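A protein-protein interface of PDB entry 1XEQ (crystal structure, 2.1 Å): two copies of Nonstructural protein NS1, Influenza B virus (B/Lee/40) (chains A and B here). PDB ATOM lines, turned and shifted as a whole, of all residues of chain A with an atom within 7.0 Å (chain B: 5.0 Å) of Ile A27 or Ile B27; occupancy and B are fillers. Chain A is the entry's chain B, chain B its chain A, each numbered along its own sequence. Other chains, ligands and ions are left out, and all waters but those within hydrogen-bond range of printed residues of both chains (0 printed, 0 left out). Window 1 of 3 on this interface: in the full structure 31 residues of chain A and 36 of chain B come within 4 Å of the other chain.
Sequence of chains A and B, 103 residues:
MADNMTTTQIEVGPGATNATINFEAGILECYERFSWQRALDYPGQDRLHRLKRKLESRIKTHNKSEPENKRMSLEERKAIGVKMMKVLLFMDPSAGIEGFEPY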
ATOM      1  N   ILE A  21     -31.785 -15.541 -29.611  1.00  0.00           N
ATOM      2  CA  ILE A  21     -31.417 -16.619 -28.718  1.00  0.00           C
ATOM      3  C   ILE A  21     -30.420 -17.591 -29.399  1.00  0.00           C
ATOM      4  O   ILE A  21     -29.415 -17.987 -28.800  1.00  0.00           O
ATOM      5  CB  ILE A  21     -32.656 -17.374 -28.271  1.00  0.00           C
ATOM      6  CG1 ILE A  21     -33.519 -16.517 -27.354  1.00  0.00           C
ATOM      7  CG2 ILE A  21     -32.274 -18.586 -27.526  1.00  0.00           C
ATOM      8  CD1 ILE A  21     -34.893 -17.202 -27.149  1.00  0.00           C
ATOM      9  N   ASN A  22     -30.719 -17.982 -30.625  1.00  0.00           N
ATOM     10  CA  ASN A  22     -29.907 -18.973 -31.361  1.00  0.00           C
ATOM     11  C   ASN A  22     -28.559 -18.397 -31.673  1.00  0.00           C
ATOM     12  O   ASN A  22     -27.493 -19.054 -31.471  1.00  0.00           O
ATOM     13  CB  ASN A  22     -30.697 -19.420 -32.636  1.00  0.00           C
ATOM     14  CG  ASN A  22     -31.922 -20.273 -32.240  1.00  0.00           C
ATOM     15  OD1 ASN A  22     -31.968 -20.758 -31.119  1.00  0.00           O
ATOM     16  ND2 ASN A  22     -32.876 -20.449 -33.106  1.00  0.00           N
ATOM     17  N   PHE A  23     -28.601 -17.161 -32.184  1.00  0.00           N
ATOM     18  CA  PHE A  23     -27.409 -16.380 -32.436  1.00  0.00           C
ATOM     19  C   PHE A  23     -26.542 -16.320 -31.201  1.00  0.00           C
ATOM     20  O   PHE A  23     -25.318 -16.727 -31.218  1.00  0.00           O
ATOM     21  CB  PHE A  23     -27.715 -15.026 -33.075  1.00  0.00           C
ATOM     22  CG  PHE A  23     -26.534 -14.107 -33.199  1.00  0.00           C
ATOM     23  CD1 PHE A  23     -25.590 -14.293 -34.205  1.00  0.00           C
ATOM     24  CD2 PHE A  23     -26.291 -13.143 -32.267  1.00  0.00           C
ATOM     25  CE1 PHE A  23     -24.498 -13.526 -34.288  1.00  0.00           C
ATOM     26  CE2 PHE A  23     -25.184 -12.315 -32.340  1.00  0.00           C
ATOM     27  CZ  PHE A  23     -24.286 -12.495 -33.366  1.00  0.00           C
ATOM     28  N   GLU A  24     -27.114 -15.889 -30.088  1.00  0.00           N
ATOM     29  CA  GLU A  24     -26.299 -15.775 -28.913  1.00  0.00           C
ATOM     30  C   GLU A  24     -25.798 -17.098 -28.383  1.00  0.00           C
ATOM     31  O   GLU A  24     -24.760 -17.155 -27.733  1.00  0.00           O
ATOM     32  CB  GLU A  24     -26.987 -14.945 -27.809  1.00  0.00           C
ATOM     33  CG  GLU A  24     -27.149 -13.530 -28.236  1.00  0.00           C
ATOM     34  CD  GLU A  24     -27.980 -12.666 -27.269  1.00  0.00           C
ATOM     35  OE1 GLU A  24     -28.654 -13.181 -26.423  1.00  0.00           O
ATOM     36  OE2 GLU A  24     -27.948 -11.457 -27.410  1.00  0.00           O
ATOM     37  N   ALA A  25     -26.507 -18.179 -28.630  1.00  0.00           N
ATOM     38  CA  ALA A  25     -25.998 -19.497 -28.268  1.00  0.00           C
ATOM     39  C   ALA A  25     -24.730 -19.865 -29.131  1.00  0.00           C
ATOM     40  O   ALA A  25     -23.786 -20.397 -28.614  1.00  0.00           O
ATOM     41  CB  ALA A  25     -27.074 -20.507 -28.423  1.00  0.00           C
ATOM     42  N   GLY A  26     -24.698 -19.458 -30.391  1.00  0.00           N
ATOM     43  CA  GLY A  26     -23.513 -19.493 -31.224  1.00  0.00           C
ATOM     44  C   GLY A  26     -22.396 -18.641 -30.687  1.00  0.00           C
ATOM     45  O   GLY A  26     -21.243 -19.063 -30.701  1.00  0.00           O
ATOM     46  N   ILE A  27     -22.722 -17.429 -30.182  1.00  0.00           N
ATOM     47  CA  ILE A  27     -21.741 -16.561 -29.520  1.00  0.00           C
ATOM     48  C   ILE A  27     -21.106 -17.226 -28.307  1.00  0.00           C
ATOM     49  O   ILE A  27     -19.909 -17.217 -28.188  1.00  0.00           O
ATOM     50  CB  ILE A  27     -22.329 -15.140 -29.192  1.00  0.00           C
ATOM     51  CG1 ILE A  27     -22.697 -14.415 -30.474  1.00  0.00           C
ATOM     52  CG2 ILE A  27     -21.416 -14.295 -28.285  1.00  0.00           C
ATOM     53  CD1 ILE A  27     -21.550 -14.085 -31.454  1.00  0.00           C
ATOM     54  N   LEU A  28     -21.924 -17.783 -27.443  1.00  0.00           N
ATOM     55  CA  LEU A  28     -21.505 -18.492 -26.285  1.00  0.00           C
ATOM     56  C   LEU A  28     -20.529 -19.648 -26.677  1.00  0.00           C
ATOM     57  O   LEU A  28     -19.525 -19.843 -26.053  1.00  0.00           O
ATOM     58  CB  LEU A  28     -22.732 -19.008 -25.534  1.00  0.00           C
ATOM     59  CG  LEU A  28     -22.411 -20.008 -24.433  1.00  0.00           C
ATOM     60  CD1 LEU A  28     -21.544 -19.291 -23.348  1.00  0.00           C
ATOM     61  CD2 LEU A  28     -23.638 -20.718 -23.810  1.00  0.00           C
ATOM     62  N   GLU A  29     -20.866 -20.416 -27.710  1.00  0.00           N
ATOM     63  CA  GLU A  29     -20.030 -21.500 -28.168  1.00  0.00           C
ATOM     64  C   GLU A  29     -18.667 -20.969 -28.523  1.00  0.00           C
ATOM     65  O   GLU A  29     -17.669 -21.547 -28.162  1.00  0.00           O
ATOM     66  CB  GLU A  29     -20.693 -22.185 -29.356  1.00  0.00           C
ATOM     67  CG  GLU A  29     -19.943 -23.374 -29.874  1.00  0.00           C
ATOM     68  CD  GLU A  29     -19.741 -24.479 -28.837  1.00  0.00           C
ATOM     69  OE1 GLU A  29     -20.520 -24.583 -27.887  1.00  0.00           O
ATOM     70  OE2 GLU A  29     -18.817 -25.298 -29.021  1.00  0.00           O
ATOM     71  N   CYS A  30     -18.629 -19.808 -29.151  1.00  0.00           N
ATOM     72  CA  CYS A  30     -17.391 -19.212 -29.539  1.00  0.00           C
ATOM     73  C   CYS A  30     -16.559 -18.767 -28.370  1.00  0.00           C
ATOM     74  O   CYS A  30     -15.355 -18.894 -28.446  1.00  0.00           O
ATOM     75  CB  CYS A  30     -17.592 -18.028 -30.421  1.00  0.00           C
ATOM     76  SG  CYS A  30     -18.218 -18.258 -32.103  1.00  0.00           S
ATOM     77  N   TYR A  31     -17.166 -18.093 -27.379  1.00  0.00           N
ATOM     78  CA  TYR A  31     -16.472 -17.776 -26.183  1.00  0.00           C
ATOM     79  C   TYR A  31     -15.887 -19.033 -25.538  1.00  0.00           C
ATOM     80  O   TYR A  31     -14.773 -18.981 -25.073  1.00  0.00           O
ATOM     81  CB  TYR A  31     -17.352 -17.083 -25.159  1.00  0.00           C
ATOM     82  CG  TYR A  31     -17.464 -15.572 -25.313  1.00  0.00           C
ATOM     83  CD1 TYR A  31     -18.428 -15.022 -26.107  1.00  0.00           C
ATOM     84  CD2 TYR A  31     -16.692 -14.710 -24.537  1.00  0.00           C
ATOM     85  CE1 TYR A  31     -18.574 -13.587 -26.215  1.00  0.00           C
ATOM     86  CE2 TYR A  31     -16.775 -13.334 -24.662  1.00  0.00           C
ATOM     87  CZ  TYR A  31     -17.729 -12.773 -25.488  1.00  0.00           C
ATOM     88  OH  TYR A  31     -17.849 -11.411 -25.588  1.00  0.00           O
ATOM     89  N   GLU A  32     -16.670 -20.101 -25.436  1.00  0.00           N
ATOM     90  CA  GLU A  32     -16.211 -21.356 -24.915  1.00  0.00           C
ATOM     91  C   GLU A  32     -14.992 -21.928 -25.682  1.00  0.00           C
ATOM     92  O   GLU A  32     -13.996 -22.419 -25.071  1.00  0.00           O
ATOM     93  CB  GLU A  32     -17.391 -22.346 -24.932  1.00  0.00           C
ATOM     94  CG  GLU A  32     -18.424 -22.023 -23.847  1.00  0.00           C
ATOM     95  CD  GLU A  32     -19.604 -22.962 -23.784  1.00  0.00           C
ATOM     96  OE1 GLU A  32     -20.461 -22.758 -22.908  1.00  0.00           O
ATOM     97  OE2 GLU A  32     -19.747 -23.830 -24.631  1.00  0.00           O
ATOM     98  N   ARG A  33     -15.043 -21.898 -27.004  1.00  0.00           N
ATOM     99  CA  ARG A  33     -13.894 -22.365 -27.771  1.00  0.00           C
ATOM    100  C   ARG A  33     -12.638 -21.532 -27.528  1.00  0.00           C
ATOM    101  O   ARG A  33     -11.535 -22.095 -27.451  1.00  0.00           O
ATOM    102  CB  ARG A  33     -14.251 -22.482 -29.238  1.00  0.00           C
ATOM    103  CG  ARG A  33     -15.293 -23.623 -29.377  1.00  0.00           C
ATOM    104  CD  ARG A  33     -15.521 -24.094 -30.740  1.00  0.00           C
ATOM    105  NE  ARG A  33     -16.786 -24.790 -30.892  1.00  0.00           N
ATOM    106  CZ  ARG A  33     -17.213 -25.189 -32.043  1.00  0.00           C
ATOM    107  NH1 ARG A  33     -16.421 -25.045 -33.092  1.00  0.00           N
ATOM    108  NH2 ARG A  33     -18.417 -25.707 -32.161  1.00  0.00           N
ATOM    109  N   ARG A  47     -18.149 -12.333 -18.360  1.00  0.00           N
ATOM    110  CA  ARG A  47     -19.096 -12.152 -19.465  1.00  0.00           C
ATOM    111  C   ARG A  47     -19.636 -13.487 -20.091  1.00  0.00           C
ATOM    112  O   ARG A  47     -20.825 -13.639 -20.350  1.00  0.00           O
ATOM    113  CB  ARG A  47     -18.501 -11.274 -20.535  1.00  0.00           C
ATOM    114  CG  ARG A  47     -19.377 -11.287 -21.730  1.00  0.00           C
ATOM    115  CD  ARG A  47     -18.918 -10.507 -22.873  1.00  0.00           C
ATOM    116  NE  ARG A  47     -19.235  -9.199 -22.501  1.00  0.00           N
ATOM    117  CZ  ARG A  47     -20.238  -8.486 -22.983  1.00  0.00           C
ATOM    118  NH1 ARG A  47     -21.007  -8.877 -24.010  1.00  0.00           N
ATOM    119  NH2 ARG A  47     -20.412  -7.318 -22.434  1.00  0.00           N
ATOM    120  N   LEU A  51     -23.461 -14.705 -19.751  1.00  0.00           N
ATOM    121  CA  LEU A  51     -24.110 -15.057 -21.000  1.00  0.00           C
ATOM    122  C   LEU A  51     -24.803 -16.392 -20.899  1.00  0.00           C
ATOM    123  O   LEU A  51     -26.016 -16.492 -21.182  1.00  0.00           O
ATOM    124  CB  LEU A  51     -23.135 -15.037 -22.188  1.00  0.00           C
ATOM    125  CG  LEU A  51     -23.781 -15.352 -23.553  1.00  0.00           C
ATOM    126  CD1 LEU A  51     -25.154 -14.676 -23.774  1.00  0.00           C
ATOM    127  CD2 LEU A  51     -22.812 -14.998 -24.774  1.00  0.00           C
ATOM    128  N   LEU A  55     -28.821 -16.806 -21.016  1.00  0.00           N
ATOM    129  CA  LEU A  55     -29.373 -17.600 -22.111  1.00  0.00           C
ATOM    130  C   LEU A  55     -30.146 -18.834 -21.672  1.00  0.00           C
ATOM    131  O   LEU A  55     -31.204 -19.146 -22.229  1.00  0.00           O
ATOM    132  CB  LEU A  55     -28.227 -17.940 -23.064  1.00  0.00           C
ATOM    133  CG  LEU A  55     -28.376 -18.060 -24.533  1.00  0.00           C
ATOM    134  CD1 LEU A  55     -29.209 -17.099 -25.184  1.00  0.00           C
ATOM    135  CD2 LEU A  55     -26.889 -18.061 -25.083  1.00  0.00           C
ATOM    136  N   LYS A  78     -27.311 -23.822 -30.072  1.00  0.00           N
ATOM    137  CA  LYS A  78     -25.923 -23.563 -30.528  1.00  0.00           C
ATOM    138  C   LYS A  78     -25.684 -24.040 -31.956  1.00  0.00           C
ATOM    139  O   LYS A  78     -25.026 -23.402 -32.749  1.00  0.00           O
ATOM    140  CB  LYS A  78     -24.996 -24.356 -29.629  1.00  0.00           C
ATOM    141  CG  LYS A  78     -24.817 -23.813 -28.234  1.00  0.00           C
ATOM    142  CD  LYS A  78     -23.926 -24.789 -27.558  1.00  0.00           C
ATOM    143  CE  LYS A  78     -23.682 -24.334 -26.285  1.00  0.00           C
ATOM    144  NZ  LYS A  78     -22.327 -24.129 -26.367  1.00  0.00           N
ATOM    145  N   GLY A  81     -27.210 -21.494 -34.191  1.00  0.00           N
ATOM    146  CA  GLY A  81     -26.351 -20.338 -34.103  1.00  0.00           C
ATOM    147  C   GLY A  81     -25.082 -20.364 -34.906  1.00  0.00           C
ATOM    148  O   GLY A  81     -24.709 -19.382 -35.538  1.00  0.00           O
ATOM    149  N   VAL A  82     -24.422 -21.513 -34.901  1.00  0.00           N
ATOM    150  CA  VAL A  82     -23.182 -21.729 -35.671  1.00  0.00           C
ATOM    151  C   VAL A  82     -23.443 -21.790 -37.129  1.00  0.00           C
ATOM    152  O   VAL A  82     -22.652 -21.273 -37.931  1.00  0.00           O
ATOM    153  CB  VAL A  82     -22.448 -22.963 -35.068  1.00  0.00           C
ATOM    154  CG1 VAL A  82     -21.414 -23.486 -35.879  1.00  0.00           C
ATOM    155  CG2 VAL A  82     -21.897 -22.560 -33.733  1.00  0.00           C
ATOM    156  N   MET A  85     -23.802 -18.168 -37.898  1.00  0.00           N
ATOM    157  CA  MET A  85     -22.445 -17.620 -37.868  1.00  0.00           C
ATOM    158  C   MET A  85     -21.619 -17.905 -39.152  1.00  0.00           C
ATOM    159  O   MET A  85     -20.943 -16.987 -39.665  1.00  0.00           O
ATOM    160  CB  MET A  85     -21.720 -18.109 -36.605  1.00  0.00           C
ATOM    161  CG  MET A  85     -20.833 -17.116 -36.006  1.00  0.00           C
ATOM    162  SD  MET A  85     -21.842 -15.686 -35.350  1.00  0.00           S
ATOM    163  CE  MET A  85     -22.730 -16.527 -33.980  1.00  0.00           C
ATOM    164  N   PHE B  23     -10.876 -10.714 -29.929  1.00  0.00           N
ATOM    165  CA  PHE B  23     -11.891 -11.732 -30.008  1.00  0.00           C
ATOM    166  C   PHE B  23     -13.260 -11.005 -29.898  1.00  0.00           C
ATOM    167  O   PHE B  23     -14.159 -11.182 -30.753  1.00  0.00           O
ATOM    168  CB  PHE B  23     -11.737 -12.717 -28.878  1.00  0.00           C
ATOM    169  CG  PHE B  23     -12.855 -13.727 -28.796  1.00  0.00           C
ATOM    170  CD1 PHE B  23     -13.037 -14.652 -29.813  1.00  0.00           C
ATOM    171  CD2 PHE B  23     -13.803 -13.657 -27.754  1.00  0.00           C
ATOM    172  CE1 PHE B  23     -14.137 -15.529 -29.771  1.00  0.00           C
ATOM    173  CE2 PHE B  23     -14.881 -14.476 -27.707  1.00  0.00           C
ATOM    174  CZ  PHE B  23     -15.055 -15.435 -28.690  1.00  0.00           C
ATOM    175  N   GLU B  24     -13.393 -10.190 -28.844  1.00  0.00           N
ATOM    176  CA  GLU B  24     -14.605  -9.396 -28.609  1.00  0.00           C
ATOM    177  C   GLU B  24     -14.895  -8.430 -29.700  1.00  0.00           C
ATOM    178  O   GLU B  24     -16.066  -8.168 -30.016  1.00  0.00           O
ATOM    179  CB  GLU B  24     -14.542  -8.768 -27.197  1.00  0.00           C
ATOM    180  CG  GLU B  24     -14.720  -9.841 -26.117  1.00  0.00           C
ATOM    181  CD  GLU B  24     -14.780  -9.256 -24.706  1.00  0.00           C
ATOM    182  OE1 GLU B  24     -14.362  -8.098 -24.546  1.00  0.00           O
ATOM    183  OE2 GLU B  24     -15.234  -9.964 -23.779  1.00  0.00           O
ATOM    184  N   ALA B  25     -13.874  -7.937 -30.379  1.00  0.00           N
ATOM    185  CA  ALA B  25     -14.152  -7.139 -31.559  1.00  0.00           C
ATOM    186  C   ALA B  25     -14.785  -7.935 -32.740  1.00  0.00           C
ATOM    187  O   ALA B  25     -15.624  -7.393 -33.487  1.00  0.00           O
ATOM    188  CB  ALA B  25     -12.948  -6.379 -31.996  1.00  0.00           C
ATOM    189  N   GLY B  26     -14.346  -9.188 -32.945  1.00  0.00           N
ATOM    190  CA  GLY B  26     -15.040 -10.061 -33.869  1.00  0.00           C
ATOM    191  C   GLY B  26     -16.470 -10.315 -33.456  1.00  0.00           C
ATOM    192  O   GLY B  26     -17.360 -10.268 -34.279  1.00  0.00           O
ATOM    193  N   ILE B  27     -16.688 -10.601 -32.197  1.00  0.00           N
ATOM    194  CA  ILE B  27     -18.015 -10.838 -31.661  1.00  0.00           C
ATOM    195  C   ILE B  27     -18.912  -9.603 -31.985  1.00  0.00           C
ATOM    196  O   ILE B  27     -19.990  -9.724 -32.557  1.00  0.00           O
ATOM    197  CB  ILE B  27     -17.921 -11.138 -30.168  1.00  0.00           C
ATOM    198  CG1 ILE B  27     -17.225 -12.458 -29.869  1.00  0.00           C
ATOM    199  CG2 ILE B  27     -19.305 -11.052 -29.411  1.00  0.00           C
ATOM    200  CD1 ILE B  27     -17.921 -13.730 -30.209  1.00  0.00           C
ATOM    201  N   LEU B  28     -18.410  -8.392 -31.720  1.00  0.00           N
ATOM    202  CA  LEU B  28     -19.151  -7.165 -32.027  1.00  0.00           C
ATOM    203  C   LEU B  28     -19.507  -7.061 -33.482  1.00  0.00           C
ATOM    204  O   LEU B  28     -20.631  -6.722 -33.823  1.00  0.00           O
ATOM    205  CB  LEU B  28     -18.334  -5.947 -31.621  1.00  0.00           C
ATOM    206  CG  LEU B  28     -18.994  -4.613 -32.003  1.00  0.00           C
ATOM    207  CD1 LEU B  28     -20.317  -4.418 -31.280  1.00  0.00           C
ATOM    208  CD2 LEU B  28     -18.109  -3.509 -31.709  1.00  0.00           C
ATOM    209  N   GLU B  29     -18.543  -7.384 -34.366  1.00  0.00           N
ATOM    210  CA  GLU B  29     -18.783  -7.341 -35.795  1.00  0.00           C
ATOM    211  C   GLU B  29     -19.883  -8.313 -36.206  1.00  0.00           C
ATOM    212  O   GLU B  29     -20.709  -8.002 -37.046  1.00  0.00           O
ATOM    213  CB  GLU B  29     -17.437  -7.591 -36.548  1.00  0.00           C
ATOM    214  CG  GLU B  29     -17.513  -7.729 -38.046  1.00  0.00           C
ATOM    215  CD  GLU B  29     -17.950  -6.458 -38.734  1.00  0.00           C
ATOM    216  OE1 GLU B  29     -18.450  -6.545 -39.875  1.00  0.00           O
ATOM    217  OE2 GLU B  29     -17.812  -5.372 -38.128  1.00  0.00           O
ATOM    218  N   CYS B  30     -19.945  -9.456 -35.579  1.00  0.00           N
ATOM    219  CA  CYS B  30     -21.023 -10.397 -35.851  1.00  0.00           C
ATOM    220  C   CYS B  30     -22.394  -9.955 -35.371  1.00  0.00           C
ATOM    221  O   CYS B  30     -23.381 -10.168 -36.069  1.00  0.00           O
ATOM    222  CB  CYS B  30     -20.703 -11.728 -35.296  1.00  0.00           C
ATOM    223  SG  CYS B  30     -19.343 -12.542 -36.253  1.00  0.00           S
ATOM    224  N   TYR B  31     -22.445  -9.317 -34.209  1.00  0.00           N
ATOM    225  CA  TYR B  31     -23.744  -8.704 -33.720  1.00  0.00           C
ATOM    226  C   TYR B  31     -24.184  -7.701 -34.703  1.00  0.00           C
ATOM    227  O   TYR B  31     -25.337  -7.653 -35.078  1.00  0.00           O
ATOM    228  CB  TYR B  31     -23.556  -8.048 -32.375  1.00  0.00           C
ATOM    229  CG  TYR B  31     -23.747  -8.937 -31.176  1.00  0.00           C
ATOM    230  CD1 TYR B  31     -22.730  -9.672 -30.647  1.00  0.00           C
ATOM    231  CD2 TYR B  31     -24.953  -8.957 -30.517  1.00  0.00           C
ATOM    232  CE1 TYR B  31     -22.913 -10.467 -29.536  1.00  0.00           C
ATOM    233  CE2 TYR B  31     -25.149  -9.783 -29.445  1.00  0.00           C
ATOM    234  CZ  TYR B  31     -24.139 -10.477 -28.906  1.00  0.00           C
ATOM    235  OH  TYR B  31     -24.391 -11.299 -27.793  1.00  0.00           O
ATOM    236  N   LEU B  51     -21.834  -3.408 -25.688  1.00  0.00           N
ATOM    237  CA  LEU B  51     -20.558  -3.988 -26.078  1.00  0.00           C
ATOM    238  C   LEU B  51     -19.712  -3.023 -26.851  1.00  0.00           C
ATOM    239  O   LEU B  51     -18.559  -2.917 -26.534  1.00  0.00           O
ATOM    240  CB  LEU B  51     -20.749  -5.264 -26.887  1.00  0.00           C
ATOM    241  CG  LEU B  51     -19.652  -6.365 -26.788  1.00  0.00           C
ATOM    242  CD1 LEU B  51     -19.622  -7.085 -28.234  1.00  0.00           C
ATOM    243  CD2 LEU B  51     -18.236  -6.136 -26.196  1.00  0.00           C
ATOM    244  N   MET B  85     -12.671 -16.099 -34.886  1.00  0.00           N
ATOM    245  CA  MET B  85     -13.929 -16.820 -34.850  1.00  0.00           C
ATOM    246  C   MET B  85     -13.987 -17.936 -35.917  1.00  0.00           C
ATOM    247  O   MET B  85     -14.487 -19.044 -35.668  1.00  0.00           O
ATOM    248  CB  MET B  85     -15.110 -15.843 -35.076  1.00  0.00           C
ATOM    249  CG  MET B  85     -15.302 -14.906 -33.865  1.00  0.00           C
ATOM    250  SD  MET B  85     -16.589 -13.715 -34.126  1.00  0.00           S
ATOM    251  CE  MET B  85     -17.976 -14.889 -33.937  1.00  0.00           C
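The side-chain hydroxyl of Tyr A31 sits at hydrogen-bond distance from the side-chain carboxylate of Glu B24 (3.5 Å).
The backbone NH (N) of Ile B27 sits at hydrogen-bond distance from the side-chain sulfur (SD) of Met B85 (3.7 Å).
The side-chain sulfur of Cys B30 sits close to the side-chain sulfur of Met B85, at 3.7 Å.
The backbone carbonyl oxygen (O) of Gly A26 is in hydrogen-bond range of the side-chain sulfur (SG) of Cys A30 (3.4 Å).
The side-chain sulfur of Cys B30 is in hydrogen-bond range of the backbone carbonyl oxygen of Gly B26 (3.6 Å).
Cys B30 touches Phe A23 (O to CZ, 3.7 Å).
Phe A23 touches Tyr B31 (CZ to N, 3.8 Å).
Glu A24 touches Tyr B31 (CG to OH, 3.6 Å).
Ile A27 touches Ile B27.
Phe B23 touches Cys A30.
Met B85 touches Cys A30 (CE to SG, 3.8 Å).
Tyr A31 touches Phe B23 (N to CZ, 3.6 Å).
Arg A47 touches Glu B24 (CD to OE2, 3.8 Å).
Arg A47 touches Leu B51.
Of the printed residues of chain B, Glu A24 touches Tyr B31 (3.6 Å).
Ile A27 touches one residue of chain B.
Arg A33 touches none of the printed residues of chain B.
No residue of chain A comes within 4 Å of Gly B26.
Ile B27 touches just one residue of chain A: Ile A27 (3.9 Å).
Leu B28 touches none of the printed residues of chain A.
Of the printed residues of chain A, Cys B30 touches Phe A23 (3.7 Å).
The nearest residue of chain B that does not touch Ile A27 is Tyr B31 (4.1 Å).
The nearest printed residue of chain A that does not touch Glu B24 is Ile A27 (8.2 Å).
Printed residues of chain A that touch a printed residue of chain B: Phe A23, Glu A24, Ile A27, Cys A30, Tyr A31 and Arg A47.
Hydrophobic or aromatic side chains of chain A within 4 Å of the printed part of chain B: Phe A23, Ile A27 and Tyr A31.
Of the 11 printed residues of chain B, 7 touch a printed residue of chain A.
Among the printed residues, no Asp or Glu carboxylate lies within 4 Å of a Lys or Arg side-chain nitrogen of the other chain.
Phe A23 touches Cys B30, and with the chains exchanged Cys A30 touches Phe B23.
Phe A23 touches Tyr B31, and with the chains exchanged Tyr A31 touches Phe B23.
Glu A24 touches Tyr B31, and with the chains exchanged Tyr A31 touches Glu B24.
Ile B27 touches its own counterpart, Ile A27.
11 positions are printed for both chains.
Of the 10 pairs that touch across the chains among the printed residues, 7 have their exchanged pair printed and touching as well.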
